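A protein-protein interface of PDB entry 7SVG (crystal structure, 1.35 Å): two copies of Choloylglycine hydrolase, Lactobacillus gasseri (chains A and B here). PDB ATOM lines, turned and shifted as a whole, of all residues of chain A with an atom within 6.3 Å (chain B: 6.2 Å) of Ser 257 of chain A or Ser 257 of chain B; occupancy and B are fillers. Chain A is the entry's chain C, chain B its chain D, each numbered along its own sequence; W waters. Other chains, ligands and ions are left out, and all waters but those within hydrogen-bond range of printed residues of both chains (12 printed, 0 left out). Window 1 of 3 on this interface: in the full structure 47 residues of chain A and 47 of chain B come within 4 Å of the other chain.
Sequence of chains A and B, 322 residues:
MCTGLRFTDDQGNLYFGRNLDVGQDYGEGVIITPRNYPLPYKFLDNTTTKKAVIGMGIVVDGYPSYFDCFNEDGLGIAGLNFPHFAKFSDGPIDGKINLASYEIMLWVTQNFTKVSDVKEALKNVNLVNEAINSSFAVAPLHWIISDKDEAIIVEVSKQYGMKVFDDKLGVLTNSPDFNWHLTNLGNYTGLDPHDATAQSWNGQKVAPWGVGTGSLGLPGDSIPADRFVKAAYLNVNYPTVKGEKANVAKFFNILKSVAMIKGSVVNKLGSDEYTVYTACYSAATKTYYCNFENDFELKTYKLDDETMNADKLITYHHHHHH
The backbone carbonyl oxygen of Gly 220 of chain A lies within hydrogen-bond range of the side-chain amino group of Lys 230 of chain B, at 2.8 Å.
NZ of Lys 230 of chain A sits at hydrogen-bond distance from O of Gly 220 of chain B (2.9 Å).
The backbone NH (N) of Gly 220 of chain A lies close to the backbone NH (N) of Gly 220 of chain B (3.3 Å).
The backbone carbonyl oxygen of Ser 257 of chain A lies close to the backbone carbonyl oxygen of Ser 257 of chain B, at 3.5 Å.
NZ of Lys 230 of chain A sits close to OG of Ser 257 of chain A, at 3.4 Å.
The side-chain hydroxyl of Ser 257 of chain B lies close to the side-chain amino group of Lys 230 of chain B, at 3.4 Å.
Among the printed residues, merely in contact across the chains: Asn 253 of chain A with Ile 261 of chain B (3.5 Å), Ser 257 of chain A with Lys 256 of chain B (3.5 Å), Lys 256 of chain A with Ser 257 of chain B (3.6 Å), Ile 261 of chain A with Asn 253 of chain B (3.6 Å), Lys 256 of chain A with Lys 256 of chain B (3.6 Å), Ser 257 of chain A with Ile 261 of chain B (3.7 Å), Ile 261 of chain A with Ser 257 of chain B (3.8 Å), Ile 261 of chain A with Leu 234 of chain B (3.8 Å) and Leu 234 of chain A with Ile 261 of chain B (3.9 Å).
Ser 257 of chain A touches just these residues of chain B: Lys 256, Ser 257 and Ile 261.
Of the printed residues of chain A, Ser 257 of chain B touches Lys 256 (3.6 Å), Ser 257 (3.5 Å) and Ile 261 (3.8 Å).
Of the printed residues of chain B, Leu 234 of chain A touches Ile 261.
Of the printed residues of chain B, Asn 253 of chain A touches Ile 261 (3.5 Å).
The nearest residue of chain A that does not touch Ser 257 of chain B is Lys 230 of chain A (4.4 Å).
Of the 12 printed residues of chain A, 7 touch a printed residue of chain B.
Along chain A the printed residues that touch a printed residue of chain B span positions 220 to 261.
Gly 220 of chain B touches its own counterpart, Gly 220 of chain A.
Asn 253 of chain A touches Ile 261 of chain B, and with the chains exchanged Ile 261 of chain A touches Asn 253 of chain B.
Lys 256 of chain A touches its own counterpart, Lys 256 of chain B.
Ser 257 of chain A touches Ile 261 of chain B, and with the chains exchanged Ile 261 of chain A touches Ser 257 of chain B.
Positions printed for both chains: 220, 230, 234, 252, 253, 254, 255, 256, 257, 258, 259 and 261.
Water W6 lies within hydrogen-bond range of OG of Ser 257 of chain B (2.7 Å), O of Ala 259 of chain A (2.7 Å), O of Ser 257 of chain A (2.8 Å) and NZ of Lys 230 of chain B (3.2 Å).
Water W1 lies within hydrogen-bond range of the backbone carbonyl oxygen of Ser 257 of chain A (2.7 Å), the side-chain amino group of Lys 230 of chain A (2.8 Å) and the side-chain amino group of Lys 230 of chain B (2.9 Å).
Water W2 lies within hydrogen-bond range of the side-chain amide oxygen of Asn 253 of chain A (2.7 Å) and the side-chain amino group of Lys 256 of chain B (2.9 Å).
Water W8 lies within hydrogen-bond range of the backbone carbonyl oxygen (O) of Ser 257 of chain B (2.7 Å), the side-chain amino group (NZ) of Lys 230 of chain A (2.8 Å) and the side-chain amino group (NZ) of Lys 230 of chain B (2.9 Å).
Water W5 bridges the backbone carbonyl oxygen (O) of Gly 220 of chain A (2.8 Å) and the side-chain amino group (NZ) of Lys 230 of chain B (3.1 Å).
Water W4 lies within hydrogen-bond range of OD1 of Asn 253 of chain B and NZ of Lys 256 of chain A.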
ATOM      1  N   GLY A 220       6.646  -3.286  -9.134  1.00  0.00           N
ATOM      2  CA  GLY A 220       5.440  -3.812  -8.516  1.00  0.00           C
ATOM      3  C   GLY A 220       4.360  -2.778  -8.279  1.00  0.00           C
ATOM      4  O   GLY A 220       3.321  -3.085  -7.686  1.00  0.00           O
ATOM      5  N   LYS A 230       5.310  -6.042 -16.214  1.00  0.00           N
ATOM      6  CA  LYS A 230       5.112  -7.229 -15.387  1.00  0.00           C
ATOM      7  C   LYS A 230       4.103  -8.188 -16.017  1.00  0.00           C
ATOM      8  O   LYS A 230       4.333  -9.402 -16.063  1.00  0.00           O
ATOM      9  CB  LYS A 230       4.701  -6.845 -13.967  1.00  0.00           C
ATOM     10  CG  LYS A 230       4.565  -8.079 -13.086  1.00  0.00           C
ATOM     11  CD  LYS A 230       4.521  -7.744 -11.602  1.00  0.00           C
ATOM     12  CE  LYS A 230       4.230  -9.000 -10.790  1.00  0.00           C
ATOM     13  NZ  LYS A 230       4.311  -8.802  -9.297  1.00  0.00           N
ATOM     14  N   LEU A 234       5.004 -11.978 -17.072  1.00  0.00           N
ATOM     15  CA  LEU A 234       4.313 -13.124 -16.487  1.00  0.00           C
ATOM     16  C   LEU A 234       3.635 -13.960 -17.561  1.00  0.00           C
ATOM     17  O   LEU A 234       3.692 -15.195 -17.525  1.00  0.00           O
ATOM     18  CB  LEU A 234       3.273 -12.663 -15.466  1.00  0.00           C
ATOM     19  CG  LEU A 234       3.810 -11.963 -14.219  1.00  0.00           C
ATOM     20  CD1 LEU A 234       2.657 -11.611 -13.279  1.00  0.00           C
ATOM     21  CD2 LEU A 234       4.876 -12.838 -13.543  1.00  0.00           C
ATOM     22  N   PHE A 252      -6.510 -15.946 -13.666  1.00  0.00           N
ATOM     23  CA  PHE A 252      -6.693 -15.127 -12.473  1.00  0.00           C
ATOM     24  C   PHE A 252      -5.388 -14.964 -11.691  1.00  0.00           C
ATOM     25  O   PHE A 252      -5.178 -13.926 -11.051  1.00  0.00           O
ATOM     26  CB  PHE A 252      -7.790 -15.742 -11.588  1.00  0.00           C
ATOM     27  CG  PHE A 252      -9.184 -15.340 -11.992  1.00  0.00           C
ATOM     28  CD1 PHE A 252      -9.826 -15.971 -13.053  1.00  0.00           C
ATOM     29  CD2 PHE A 252      -9.837 -14.298 -11.344  1.00  0.00           C
ATOM     30  CE1 PHE A 252     -11.119 -15.580 -13.449  1.00  0.00           C
ATOM     31  CE2 PHE A 252     -11.117 -13.897 -11.730  1.00  0.00           C
ATOM     32  CZ  PHE A 252     -11.759 -14.536 -12.789  1.00  0.00           C
ATOM     33  N   ASN A 253      -4.513 -15.972 -11.718  1.00  0.00           N
ATOM     34  CA  ASN A 253      -3.222 -15.842 -11.041  1.00  0.00           C
ATOM     35  C   ASN A 253      -2.447 -14.654 -11.601  1.00  0.00           C
ATOM     36  O   ASN A 253      -1.879 -13.852 -10.850  1.00  0.00           O
ATOM     37  CB  ASN A 253      -2.392 -17.115 -11.230  1.00  0.00           C
ATOM     38  CG  ASN A 253      -2.928 -18.304 -10.465  1.00  0.00           C
ATOM     39  OD1 ASN A 253      -3.637 -18.166  -9.463  1.00  0.00           O
ATOM     40  ND2 ASN A 253      -2.569 -19.491 -10.932  1.00  0.00           N
ATOM     41  N   ILE A 254      -2.417 -14.533 -12.931  1.00  0.00           N
ATOM     42  CA  ILE A 254      -1.682 -13.443 -13.571  1.00  0.00           C
ATOM     43  C   ILE A 254      -2.352 -12.100 -13.293  1.00  0.00           C
ATOM     44  O   ILE A 254      -1.707 -11.137 -12.874  1.00  0.00           O
ATOM     45  CB  ILE A 254      -1.542 -13.702 -15.081  1.00  0.00           C
ATOM     46  CG1 ILE A 254      -0.681 -14.942 -15.346  1.00  0.00           C
ATOM     47  CG2 ILE A 254      -0.970 -12.467 -15.787  1.00  0.00           C
ATOM     48  CD1 ILE A 254      -0.792 -15.439 -16.806  1.00  0.00           C
ATOM     49  N   LEU A 255      -3.657 -12.001 -13.544  1.00  0.00           N
ATOM     50  CA  LEU A 255      -4.303 -10.703 -13.397  1.00  0.00           C
ATOM     51  C   LEU A 255      -4.369 -10.252 -11.945  1.00  0.00           C
ATOM     52  O   LEU A 255      -4.292  -9.051 -11.674  1.00  0.00           O
ATOM     53  CB  LEU A 255      -5.685 -10.701 -14.055  1.00  0.00           C
ATOM     54  CG  LEU A 255      -5.690 -10.457 -15.570  1.00  0.00           C
ATOM     55  CD1 LEU A 255      -7.099 -10.069 -16.052  1.00  0.00           C
ATOM     56  CD2 LEU A 255      -4.661  -9.416 -15.985  1.00  0.00           C
ATOM     57  N   LYS A 256      -4.508 -11.188 -10.993  1.00  0.00           N
ATOM     58  CA  LYS A 256      -4.512 -10.768  -9.598  1.00  0.00           C
ATOM     59  C   LYS A 256      -3.125 -10.339  -9.148  1.00  0.00           C
ATOM     60  O   LYS A 256      -3.001  -9.492  -8.256  1.00  0.00           O
ATOM     61  CB  LYS A 256      -5.057 -11.864  -8.681  1.00  0.00           C
ATOM     62  CG  LYS A 256      -6.556 -12.152  -8.900  1.00  0.00           C
ATOM     63  CD  LYS A 256      -7.385 -10.879  -8.739  1.00  0.00           C
ATOM     64  CE  LYS A 256      -8.889 -11.160  -8.631  1.00  0.00           C
ATOM     65  NZ  LYS A 256      -9.651  -9.862  -8.586  1.00  0.00           N
ATOM     66  N   SER A 257      -2.078 -10.881  -9.778  1.00  0.00           N
ATOM     67  CA  SER A 257      -0.725 -10.430  -9.469  1.00  0.00           C
ATOM     68  C   SER A 257      -0.543  -8.957  -9.821  1.00  0.00           C
ATOM     69  O   SER A 257       0.164  -8.226  -9.114  1.00  0.00           O
ATOM     70  CB  SER A 257       0.292 -11.285 -10.225  1.00  0.00           C
ATOM     71  OG  SER A 257       1.612 -10.781 -10.044  1.00  0.00           O
ATOM     72  N   VAL A 258      -1.147  -8.501 -10.919  1.00  0.00           N
ATOM     73  CA  VAL A 258      -0.972  -7.109 -11.364  1.00  0.00           C
ATOM     74  C   VAL A 258      -2.177  -6.231 -11.021  1.00  0.00           C
ATOM     75  O   VAL A 258      -2.318  -5.129 -11.553  1.00  0.00           O
ATOM     76  CB  VAL A 258      -0.568  -6.991 -12.842  1.00  0.00           C
ATOM     77  CG1 VAL A 258       0.798  -7.605 -13.063  1.00  0.00           C
ATOM     78  CG2 VAL A 258      -1.610  -7.629 -13.746  1.00  0.00           C
ATOM     79  N   ALA A 259      -3.043  -6.691 -10.129  1.00  0.00           N
ATOM     80  CA  ALA A 259      -4.182  -5.885  -9.721  1.00  0.00           C
ATOM     81  C   ALA A 259      -3.735  -4.608  -9.006  1.00  0.00           C
ATOM     82  O   ALA A 259      -2.667  -4.557  -8.386  1.00  0.00           O
ATOM     83  CB  ALA A 259      -5.108  -6.717  -8.831  1.00  0.00           C
ATOM     84  N   ILE A 261      -4.345  -2.484  -5.926  1.00  0.00           N
ATOM     85  CA  ILE A 261      -4.848  -2.877  -4.617  1.00  0.00           C
ATOM     86  C   ILE A 261      -5.425  -1.666  -3.890  1.00  0.00           C
ATOM     87  O   ILE A 261      -4.776  -0.616  -3.788  1.00  0.00           O
ATOM     88  CB  ILE A 261      -3.736  -3.552  -3.802  1.00  0.00           C
ATOM     89  CG1 ILE A 261      -3.179  -4.733  -4.599  1.00  0.00           C
ATOM     90  CG2 ILE A 261      -4.267  -3.987  -2.446  1.00  0.00           C
ATOM     91  CD1 ILE A 261      -4.228  -5.741  -5.037  1.00  0.00           C
ATOM     92  N   GLY B 220       8.352  -5.546  -7.489  1.00  0.00           N
ATOM     93  CA  GLY B 220       7.347  -6.517  -7.867  1.00  0.00           C
ATOM     94  C   GLY B 220       7.857  -7.935  -8.059  1.00  0.00           C
ATOM     95  O   GLY B 220       7.084  -8.819  -8.438  1.00  0.00           O
ATOM     96  N   LYS B 230       6.357  -5.028  -0.064  1.00  0.00           N
ATOM     97  CA  LYS B 230       5.069  -4.841  -0.731  1.00  0.00           C
ATOM     98  C   LYS B 230       3.903  -5.324   0.133  1.00  0.00           C
ATOM     99  O   LYS B 230       2.882  -4.637   0.243  1.00  0.00           O
ATOM    100  CB  LYS B 230       5.068  -5.504  -2.110  1.00  0.00           C
ATOM    101  CG  LYS B 230       3.744  -5.278  -2.839  1.00  0.00           C
ATOM    102  CD  LYS B 230       3.819  -5.540  -4.351  1.00  0.00           C
ATOM    103  CE  LYS B 230       2.437  -5.294  -5.000  1.00  0.00           C
ATOM    104  NZ  LYS B 230       2.438  -5.513  -6.488  1.00  0.00           N
ATOM    105  N   LEU B 234       0.957  -2.838   1.381  1.00  0.00           N
ATOM    106  CA  LEU B 234      -0.438  -3.086   1.024  1.00  0.00           C
ATOM    107  C   LEU B 234      -1.311  -3.244   2.261  1.00  0.00           C
ATOM    108  O   LEU B 234      -2.412  -2.684   2.332  1.00  0.00           O
ATOM    109  CB  LEU B 234      -0.550  -4.327   0.144  1.00  0.00           C
ATOM    110  CG  LEU B 234       0.080  -4.248  -1.247  1.00  0.00           C
ATOM    111  CD1 LEU B 234      -0.235  -5.523  -2.003  1.00  0.00           C
ATOM    112  CD2 LEU B 234      -0.414  -3.015  -2.019  1.00  0.00           C
ATOM    113  N   PHE B 252      -7.549 -12.122   0.141  1.00  0.00           N
ATOM    114  CA  PHE B 252      -7.050 -12.724  -1.088  1.00  0.00           C
ATOM    115  C   PHE B 252      -6.524 -11.671  -2.063  1.00  0.00           C
ATOM    116  O   PHE B 252      -5.577 -11.945  -2.809  1.00  0.00           O
ATOM    117  CB  PHE B 252      -8.150 -13.575  -1.731  1.00  0.00           C
ATOM    118  CG  PHE B 252      -8.256 -14.949  -1.139  1.00  0.00           C
ATOM    119  CD1 PHE B 252      -8.927 -15.160   0.059  1.00  0.00           C
ATOM    120  CD2 PHE B 252      -7.628 -16.031  -1.753  1.00  0.00           C
ATOM    121  CE1 PHE B 252      -8.987 -16.444   0.627  1.00  0.00           C
ATOM    122  CE2 PHE B 252      -7.695 -17.310  -1.204  1.00  0.00           C
ATOM    123  CZ  PHE B 252      -8.366 -17.511  -0.009  1.00  0.00           C
ATOM    124  N   ASN B 253      -7.111 -10.472  -2.072  1.00  0.00           N
ATOM    125  CA  ASN B 253      -6.597  -9.424  -2.956  1.00  0.00           C
ATOM    126  C   ASN B 253      -5.140  -9.129  -2.625  1.00  0.00           C
ATOM    127  O   ASN B 253      -4.293  -9.017  -3.526  1.00  0.00           O
ATOM    128  CB  ASN B 253      -7.417  -8.141  -2.798  1.00  0.00           C
ATOM    129  CG  ASN B 253      -8.832  -8.268  -3.308  1.00  0.00           C
ATOM    130  OD1 ASN B 253      -9.124  -9.088  -4.187  1.00  0.00           O
ATOM    131  ND2 ASN B 253      -9.724  -7.433  -2.770  1.00  0.00           N
ATOM    132  N   ILE B 254      -4.823  -9.023  -1.331  1.00  0.00           N
ATOM    133  CA  ILE B 254      -3.456  -8.714  -0.924  1.00  0.00           C
ATOM    134  C   ILE B 254      -2.532  -9.889  -1.222  1.00  0.00           C
ATOM    135  O   ILE B 254      -1.463  -9.722  -1.816  1.00  0.00           O
ATOM    136  CB  ILE B 254      -3.416  -8.310   0.563  1.00  0.00           C
ATOM    137  CG1 ILE B 254      -4.193  -7.008   0.807  1.00  0.00           C
ATOM    138  CG2 ILE B 254      -1.967  -8.218   1.065  1.00  0.00           C
ATOM    139  CD1 ILE B 254      -4.502  -6.739   2.290  1.00  0.00           C
ATOM    140  N   LEU B 255      -2.906 -11.100  -0.792  1.00  0.00           N
ATOM    141  CA  LEU B 255      -1.970 -12.208  -0.967  1.00  0.00           C
ATOM    142  C   LEU B 255      -1.797 -12.605  -2.431  1.00  0.00           C
ATOM    143  O   LEU B 255      -0.707 -13.044  -2.825  1.00  0.00           O
ATOM    144  CB  LEU B 255      -2.354 -13.413  -0.105  1.00  0.00           C
ATOM    145  CG  LEU B 255      -1.936 -13.338   1.371  1.00  0.00           C
ATOM    146  CD1 LEU B 255      -2.120 -14.695   2.049  1.00  0.00           C
ATOM    147  CD2 LEU B 255      -0.493 -12.856   1.549  1.00  0.00           C
ATOM    148  N   LYS B 256      -2.844 -12.474  -3.255  1.00  0.00           N
ATOM    149  CA  LYS B 256      -2.653 -12.773  -4.672  1.00  0.00           C
ATOM    150  C   LYS B 256      -1.797 -11.723  -5.364  1.00  0.00           C
ATOM    151  O   LYS B 256      -1.123 -12.046  -6.343  1.00  0.00           O
ATOM    152  CB  LYS B 256      -3.996 -12.968  -5.379  1.00  0.00           C
ATOM    153  CG  LYS B 256      -4.750 -14.196  -4.865  1.00  0.00           C
ATOM    154  CD  LYS B 256      -3.936 -15.483  -5.028  1.00  0.00           C
ATOM    155  CE  LYS B 256      -4.827 -16.724  -4.888  1.00  0.00           C
ATOM    156  NZ  LYS B 256      -4.008 -17.975  -4.984  1.00  0.00           N
ATOM    157  N   SER B 257      -1.780 -10.489  -4.843  1.00  0.00           N
ATOM    158  CA  SER B 257      -0.902  -9.448  -5.383  1.00  0.00           C
ATOM    159  C   SER B 257       0.565  -9.822  -5.222  1.00  0.00           C
ATOM    160  O   SER B 257       1.381  -9.540  -6.108  1.00  0.00           O
ATOM    161  CB  SER B 257      -1.188  -8.109  -4.699  1.00  0.00           C
ATOM    162  OG  SER B 257      -0.260  -7.092  -5.083  1.00  0.00           O
ATOM    163  N   VAL B 258       0.925 -10.439  -4.092  1.00  0.00           N
ATOM    164  CA  VAL B 258       2.308 -10.823  -3.811  1.00  0.00           C
ATOM    165  C   VAL B 258       2.570 -12.310  -4.043  1.00  0.00           C
ATOM    166  O   VAL B 258       3.598 -12.831  -3.603  1.00  0.00           O
ATOM    167  CB  VAL B 258       2.764 -10.369  -2.416  1.00  0.00           C
ATOM    168  CG1 VAL B 258       2.711  -8.852  -2.347  1.00  0.00           C
ATOM    169  CG2 VAL B 258       1.914 -11.027  -1.305  1.00  0.00           C
ATOM    170  N   ALA B 259       1.676 -13.005  -4.741  1.00  0.00           N
ATOM    171  CA  ALA B 259       1.908 -14.400  -5.070  1.00  0.00           C
ATOM    172  C   ALA B 259       3.131 -14.566  -5.964  1.00  0.00           C
ATOM    173  O   ALA B 259       3.529 -13.665  -6.701  1.00  0.00           O
ATOM    174  CB  ALA B 259       0.684 -14.975  -5.782  1.00  0.00           C
ATOM    175  N   ILE B 261       4.448 -16.213  -9.107  1.00  0.00           N
ATOM    176  CA  ILE B 261       3.660 -16.638 -10.266  1.00  0.00           C
ATOM    177  C   ILE B 261       4.432 -17.687 -11.057  1.00  0.00           C
ATOM    178  O   ILE B 261       5.610 -17.497 -11.390  1.00  0.00           O
ATOM    179  CB  ILE B 261       3.303 -15.429 -11.148  1.00  0.00           C
ATOM    180  CG1 ILE B 261       2.549 -14.368 -10.333  1.00  0.00           C
ATOM    181  CG2 ILE B 261       2.509 -15.875 -12.368  1.00  0.00           C
ATOM    182  CD1 ILE B 261       1.281 -14.890  -9.639  1.00  0.00           C
HETATM  183  O   HOH W   1       2.414  -6.719  -9.076  1.00  0.00           O
HETATM  184  O   HOH W   2      -4.394 -19.622  -7.281  1.00  0.00           O
HETATM  185  O   HOH W   3      -2.086 -17.065  -7.424  1.00  0.00           O
HETATM  186  O   HOH W   4      -7.861  -8.244  -6.592  1.00  0.00           O
HETATM  187  O   HOH W   5       0.664  -2.979  -6.785  1.00  0.00           O
HETATM  188  O   HOH W   6      -0.523  -6.010  -7.498  1.00  0.00           O
HETATM  189  O   HOH W   7       2.926 -11.159  -7.792  1.00  0.00           O
HETATM  190  O   HOH W   8       3.701  -8.161  -6.592  1.00  0.00           O
HETATM  191  O   HOH W   9      -5.152  -9.169  -6.282  1.00  0.00           O
HETATM  192  O   HOH W  10       6.203 -11.424  -8.945  1.00  0.00           O
HETATM  193  O   HOH W  11      -1.948 -14.283  -8.010  1.00  0.00           O
HETATM  194  O   HOH W  12     -10.968  -9.413  -6.134  1.00  0.00           O
